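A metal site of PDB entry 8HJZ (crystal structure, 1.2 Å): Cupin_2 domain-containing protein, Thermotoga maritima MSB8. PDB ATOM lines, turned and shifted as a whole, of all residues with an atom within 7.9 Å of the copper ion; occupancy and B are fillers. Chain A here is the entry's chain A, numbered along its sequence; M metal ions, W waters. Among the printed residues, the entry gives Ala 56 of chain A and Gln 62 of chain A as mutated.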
ATOM      1  N   ARG A  43     -11.681  30.930 -15.760  1.00  0.00           N
ATOM      2  CA  ARG A  43     -12.061  30.718 -17.138  1.00  0.00           C
ATOM      3  C   ARG A  43     -12.295  29.220 -17.389  1.00  0.00           C
ATOM      4  O   ARG A  43     -11.704  28.371 -16.744  1.00  0.00           O
ATOM      5  CB  ARG A  43     -11.002  31.257 -18.108  1.00  0.00           C
ATOM      6  CG  ARG A  43     -10.733  32.739 -18.019  1.00  0.00           C
ATOM      7  CD  ARG A  43      -9.675  33.124 -17.014  1.00  0.00           C
ATOM      8  NE  ARG A  43      -8.404  32.478 -17.241  1.00  0.00           N
ATOM      9  CZ  ARG A  43      -7.443  32.873 -18.052  1.00  0.00           C
ATOM     10  NH1 ARG A  43      -6.307  32.192 -18.178  1.00  0.00           N
ATOM     11  NH2 ARG A  43      -7.615  33.982 -18.762  1.00  0.00           N
ATOM     12  N   ILE A  53      -2.578  25.495 -28.008  1.00  0.00           N
ATOM     13  CA  ILE A  53      -2.095  26.629 -27.246  1.00  0.00           C
ATOM     14  C   ILE A  53      -0.592  26.409 -27.206  1.00  0.00           C
ATOM     15  O   ILE A  53      -0.092  25.631 -26.381  1.00  0.00           O
ATOM     16  CB  ILE A  53      -2.739  26.649 -25.851  1.00  0.00           C
ATOM     17  CG1 ILE A  53      -4.259  26.777 -25.949  1.00  0.00           C
ATOM     18  CG2 ILE A  53      -2.150  27.734 -24.955  1.00  0.00           C
ATOM     19  CD1 ILE A  53      -5.030  26.609 -24.659  1.00  0.00           C
ATOM     20  N   ASP A  54       0.152  27.086 -28.074  1.00  0.00           N
ATOM     21  CA  ASP A  54       1.563  26.698 -28.239  1.00  0.00           C
ATOM     22  C   ASP A  54       2.406  27.197 -27.066  1.00  0.00           C
ATOM     23  O   ASP A  54       2.009  28.061 -26.288  1.00  0.00           O
ATOM     24  CB  ASP A  54       2.137  27.192 -29.562  1.00  0.00           C
ATOM     25  CG  ASP A  54       3.193  26.256 -30.124  1.00  0.00           C
ATOM     26  OD1 ASP A  54       3.669  25.332 -29.443  1.00  0.00           O
ATOM     27  OD2 ASP A  54       3.575  26.455 -31.280  1.00  0.00           O
ATOM     28  N   ARG A  55       3.581  26.605 -26.954  1.00  0.00           N
ATOM     29  CA  ARG A  55       4.473  26.872 -25.825  1.00  0.00           C
ATOM     30  C   ARG A  55       4.708  28.366 -25.644  1.00  0.00           C
ATOM     31  O   ARG A  55       5.036  29.097 -26.566  1.00  0.00           O
ATOM     32  CB  ARG A  55       5.801  26.165 -26.019  1.00  0.00           C
ATOM     33  CG  ARG A  55       5.755  24.657 -25.804  1.00  0.00           C
ATOM     34  CD  ARG A  55       7.140  24.049 -26.020  1.00  0.00           C
ATOM     35  NE  ARG A  55       7.162  22.643 -25.717  1.00  0.00           N
ATOM     36  CZ  ARG A  55       6.837  21.656 -26.509  1.00  0.00           C
ATOM     37  NH1 ARG A  55       6.461  21.869 -27.775  1.00  0.00           N
ATOM     38  NH2 ARG A  55       6.910  20.409 -26.020  1.00  0.00           N
ATOM     39  N   ALA A  56       4.583  28.775 -24.405  1.00  0.00           N
ATOM     40  CA  ALA A  56       4.777  30.152 -23.993  1.00  0.00           C
ATOM     41  C   ALA A  56       5.134  30.173 -22.533  1.00  0.00           C
ATOM     42  O   ALA A  56       5.036  29.190 -21.803  1.00  0.00           O
ATOM     43  CB  ALA A  56       3.499  30.981 -24.251  1.00  0.00           C
ATOM     44  N   SER A  57       5.526  31.379 -22.083  1.00  0.00           N
ATOM     45  CA  SER A  57       5.701  31.586 -20.660  1.00  0.00           C
ATOM     46  C   SER A  57       5.248  33.025 -20.346  1.00  0.00           C
ATOM     47  O   SER A  57       5.183  33.839 -21.240  1.00  0.00           O
ATOM     48  CB  SER A  57       7.114  31.391 -20.183  1.00  0.00           C
ATOM     49  OG  SER A  57       8.012  32.277 -20.783  1.00  0.00           O
ATOM     50  N   HIS A  58       4.943  33.250 -19.080  1.00  0.00           N
ATOM     51  CA  HIS A  58       4.449  34.573 -18.656  1.00  0.00           C
ATOM     52  C   HIS A  58       4.768  34.739 -17.180  1.00  0.00           C
ATOM     53  O   HIS A  58       4.916  33.767 -16.455  1.00  0.00           O
ATOM     54  CB  HIS A  58       2.975  34.840 -18.883  1.00  0.00           C
ATOM     55  CG  HIS A  58       2.133  33.620 -18.719  1.00  0.00           C
ATOM     56  ND1 HIS A  58       1.921  33.003 -17.508  1.00  0.00           N
ATOM     57  CD2 HIS A  58       1.451  32.896 -19.617  1.00  0.00           C
ATOM     58  CE1 HIS A  58       1.109  31.943 -17.702  1.00  0.00           C
ATOM     59  NE2 HIS A  58       0.791  31.850 -18.979  1.00  0.00           N
ATOM     60  N   TRP A  60       3.263  35.259 -14.447  1.00  0.00           N
ATOM     61  CA  TRP A  60       2.267  34.838 -13.467  1.00  0.00           C
ATOM     62  C   TRP A  60       2.099  33.323 -13.591  1.00  0.00           C
ATOM     63  O   TRP A  60       2.344  32.728 -14.641  1.00  0.00           O
ATOM     64  CB  TRP A  60       0.938  35.551 -13.634  1.00  0.00           C
ATOM     65  CG  TRP A  60       0.303  35.404 -14.979  1.00  0.00           C
ATOM     66  CD1 TRP A  60      -0.515  34.410 -15.427  1.00  0.00           C
ATOM     67  CD2 TRP A  60       0.479  36.323 -16.079  1.00  0.00           C
ATOM     68  NE1 TRP A  60      -0.865  34.644 -16.732  1.00  0.00           N
ATOM     69  CE2 TRP A  60      -0.279  35.815 -17.155  1.00  0.00           C
ATOM     70  CE3 TRP A  60       1.174  37.516 -16.252  1.00  0.00           C
ATOM     71  CZ2 TRP A  60      -0.347  36.475 -18.375  1.00  0.00           C
ATOM     72  CZ3 TRP A  60       1.126  38.179 -17.452  1.00  0.00           C
ATOM     73  CH2 TRP A  60       0.364  37.648 -18.510  1.00  0.00           C
ATOM     74  N   GLU A  61       1.647  32.756 -12.459  1.00  0.00           N
ATOM     75  CA  GLU A  61       1.318  31.345 -12.378  1.00  0.00           C
ATOM     76  C   GLU A  61      -0.017  31.036 -13.007  1.00  0.00           C
ATOM     77  O   GLU A  61      -0.814  31.926 -13.251  1.00  0.00           O
ATOM     78  CB  GLU A  61       1.238  30.901 -10.912  1.00  0.00           C
ATOM     79  CG  GLU A  61       0.079  31.391 -10.110  1.00  0.00           C
ATOM     80  CD  GLU A  61       0.175  32.787  -9.533  1.00  0.00           C
ATOM     81  OE1 GLU A  61       1.077  33.613  -9.948  1.00  0.00           O
ATOM     82  OE2 GLU A  61      -0.686  33.087  -8.667  1.00  0.00           O
ATOM     83  N   GLN A  62      -0.277  29.757 -13.216  1.00  0.00           N
ATOM     84  CA  GLN A  62      -1.536  29.273 -13.774  1.00  0.00           C
ATOM     85  C   GLN A  62      -1.935  28.014 -13.033  1.00  0.00           C
ATOM     86  O   GLN A  62      -1.113  27.147 -12.747  1.00  0.00           O
ATOM     87  CB  GLN A  62      -1.332  29.036 -15.270  1.00  0.00           C
ATOM     88  CG  GLN A  62      -2.463  28.937 -16.205  1.00  0.00           C
ATOM     89  CD  GLN A  62      -1.980  29.099 -17.659  1.00  0.00           C
ATOM     90  OE1 GLN A  62      -1.196  29.947 -18.079  1.00  0.00           O
ATOM     91  NE2 GLN A  62      -2.526  28.210 -18.436  1.00  0.00           N
ATOM     92  N   ILE A  64      -4.818  24.891 -13.184  1.00  0.00           N
ATOM     93  CA  ILE A  64      -5.705  24.244 -14.139  1.00  0.00           C
ATOM     94  C   ILE A  64      -6.337  23.009 -13.520  1.00  0.00           C
ATOM     95  O   ILE A  64      -5.655  22.287 -12.774  1.00  0.00           O
ATOM     96  CB  ILE A  64      -4.923  23.851 -15.404  1.00  0.00           C
ATOM     97  CG1 ILE A  64      -4.509  25.127 -16.164  1.00  0.00           C
ATOM     98  CG2 ILE A  64      -5.656  22.883 -16.284  1.00  0.00           C
ATOM     99  CD1 ILE A  64      -3.567  24.875 -17.299  1.00  0.00           C
ATOM    100  N   VAL A  90       1.339  25.566 -12.936  1.00  0.00           N
ATOM    101  CA  VAL A  90       2.418  26.103 -13.725  1.00  0.00           C
ATOM    102  C   VAL A  90       3.020  27.298 -12.960  1.00  0.00           C
ATOM    103  O   VAL A  90       2.340  28.297 -12.774  1.00  0.00           O
ATOM    104  CB  VAL A  90       1.948  26.563 -15.115  1.00  0.00           C
ATOM    105  CG1 VAL A  90       3.143  26.892 -16.008  1.00  0.00           C
ATOM    106  CG2 VAL A  90       1.055  25.534 -15.806  1.00  0.00           C
ATOM    107  N   GLU A  94       7.415  29.470 -16.258  1.00  0.00           N
ATOM    108  CA  GLU A  94       7.644  28.097 -16.761  1.00  0.00           C
ATOM    109  C   GLU A  94       7.041  27.950 -18.127  1.00  0.00           C
ATOM    110  O   GLU A  94       5.913  28.358 -18.349  1.00  0.00           O
ATOM    111  CB  GLU A  94       7.027  27.086 -15.759  1.00  0.00           C
ATOM    112  CG  GLU A  94       7.247  25.630 -16.179  1.00  0.00           C
ATOM    113  CD  GLU A  94       8.701  25.236 -15.984  1.00  0.00           C
ATOM    114  OE1 GLU A  94       9.253  24.410 -16.752  1.00  0.00           O
ATOM    115  OE2 GLU A  94       9.384  25.796 -15.092  1.00  0.00           O
ATOM    116  N   ILE A  95       7.767  27.331 -19.051  1.00  0.00           N
ATOM    117  CA  ILE A  95       7.239  27.054 -20.381  1.00  0.00           C
ATOM    118  C   ILE A  95       6.132  26.017 -20.333  1.00  0.00           C
ATOM    119  O   ILE A  95       6.201  24.989 -19.662  1.00  0.00           O
ATOM    120  CB  ILE A  95       8.394  26.576 -21.302  1.00  0.00           C
ATOM    121  CG1 ILE A  95       9.374  27.741 -21.595  1.00  0.00           C
ATOM    122  CG2 ILE A  95       7.859  26.002 -22.591  1.00  0.00           C
ATOM    123  CD1 ILE A  95      10.679  27.322 -22.223  1.00  0.00           C
ATOM    124  N   HIS A  96       5.040  26.288 -21.042  1.00  0.00           N
ATOM    125  CA  HIS A  96       3.899  25.382 -21.041  1.00  0.00           C
ATOM    126  C   HIS A  96       3.070  25.672 -22.278  1.00  0.00           C
ATOM    127  O   HIS A  96       3.057  26.764 -22.824  1.00  0.00           O
ATOM    128  CB  HIS A  96       3.015  25.574 -19.793  1.00  0.00           C
ATOM    129  CG  HIS A  96       2.460  26.969 -19.712  1.00  0.00           C
ATOM    130  ND1 HIS A  96       3.223  28.055 -19.384  1.00  0.00           N
ATOM    131  CD2 HIS A  96       1.237  27.508 -19.929  1.00  0.00           C
ATOM    132  CE1 HIS A  96       2.496  29.156 -19.398  1.00  0.00           C
ATOM    133  NE2 HIS A  96       1.267  28.874 -19.725  1.00  0.00           N
ATOM    134  N   GLY A  97       2.339  24.659 -22.720  1.00  0.00           N
ATOM    135  CA  GLY A  97       1.332  24.798 -23.746  1.00  0.00           C
ATOM    136  C   GLY A  97       0.462  23.566 -23.733  1.00  0.00           C
ATOM    137  O   GLY A  97       0.662  22.669 -22.902  1.00  0.00           O
ATOM    138  N   PHE A  98      -0.511  23.492 -24.620  1.00  0.00           N
ATOM    139  CA  PHE A  98      -1.548  22.465 -24.603  1.00  0.00           C
ATOM    140  C   PHE A  98      -1.970  22.133 -26.032  1.00  0.00           C
ATOM    141  O   PHE A  98      -1.978  22.968 -26.885  1.00  0.00           O
ATOM    142  CB  PHE A  98      -2.796  22.903 -23.814  1.00  0.00           C
ATOM    143  CG  PHE A  98      -2.391  23.381 -22.431  1.00  0.00           C
ATOM    144  CD1 PHE A  98      -2.094  22.510 -21.419  1.00  0.00           C
ATOM    145  CD2 PHE A  98      -2.275  24.736 -22.201  1.00  0.00           C
ATOM    146  CE1 PHE A  98      -1.695  22.969 -20.158  1.00  0.00           C
ATOM    147  CE2 PHE A  98      -1.910  25.207 -20.948  1.00  0.00           C
ATOM    148  CZ  PHE A  98      -1.591  24.333 -19.946  1.00  0.00           C
ATOM    149  N   CSD A 110      -9.206  27.170 -15.892  1.00  0.00           N
ATOM    150  CA  CSD A 110      -7.893  27.847 -15.859  1.00  0.00           C
ATOM    151  CB  CSD A 110      -7.437  28.196 -17.284  1.00  0.00           C
ATOM    152  SG  CSD A 110      -5.774  28.796 -17.339  1.00  0.00           S
ATOM    153  C   CSD A 110      -8.072  29.147 -15.044  1.00  0.00           C
ATOM    154  O   CSD A 110      -8.935  29.932 -15.336  1.00  0.00           O
ATOM    155  OD1 CSD A 110      -5.317  28.742 -18.974  1.00  0.00           O
ATOM    156  OD2 CSD A 110      -5.865  30.155 -16.962  1.00  0.00           O
ATOM    157  N   ILE A 112      -5.880  32.352 -13.108  1.00  0.00           N
ATOM    158  CA  ILE A 112      -4.657  33.137 -13.042  1.00  0.00           C
ATOM    159  C   ILE A 112      -4.932  34.329 -12.114  1.00  0.00           C
ATOM    160  O   ILE A 112      -6.070  34.779 -11.980  1.00  0.00           O
ATOM    161  CB  ILE A 112      -4.208  33.636 -14.422  1.00  0.00           C
ATOM    162  CG1 ILE A 112      -5.237  34.504 -15.134  1.00  0.00           C
ATOM    163  CG2 ILE A 112      -3.740  32.457 -15.294  1.00  0.00           C
ATOM    164  CD1 ILE A 112      -4.763  35.147 -16.441  1.00  0.00           C
HETATM  165 CU    CU M   1      -0.140  30.291 -19.862  1.00  0.00          CU
HETATM  166  O   HOH W   1      -1.454  29.334 -21.288  1.00  0.00           O
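The backbone carbonyl oxygen (O) of His 96 lies within hydrogen-bond range of the backbone NH (N) of Ala 56.
A ring nitrogen (ND1) of His 96 is in hydrogen-bond range of the backbone carbonyl oxygen of Glu 94.
The backbone carbonyl oxygen of Trp 60 is in hydrogen-bond range of a ring nitrogen (ND1) of His 58, at 2.9 Å.
NE2 of Gln 62 sits at hydrogen-bond distance from OD1 of CSD 110, at 2.9 Å.
The backbone carbonyl oxygen of Gln 62 is in hydrogen-bond range of the backbone NH of Val 90.
The copper ion is bound by a ring nitrogen (NE2) of His 96, a ring nitrogen (NE2) of His 58, the side-chain amide oxygen (OE1) of Gln 62 and water W1.
Three residues have an atom within 4 Å of the copper ion: His 58, Gln 62 and His 96.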
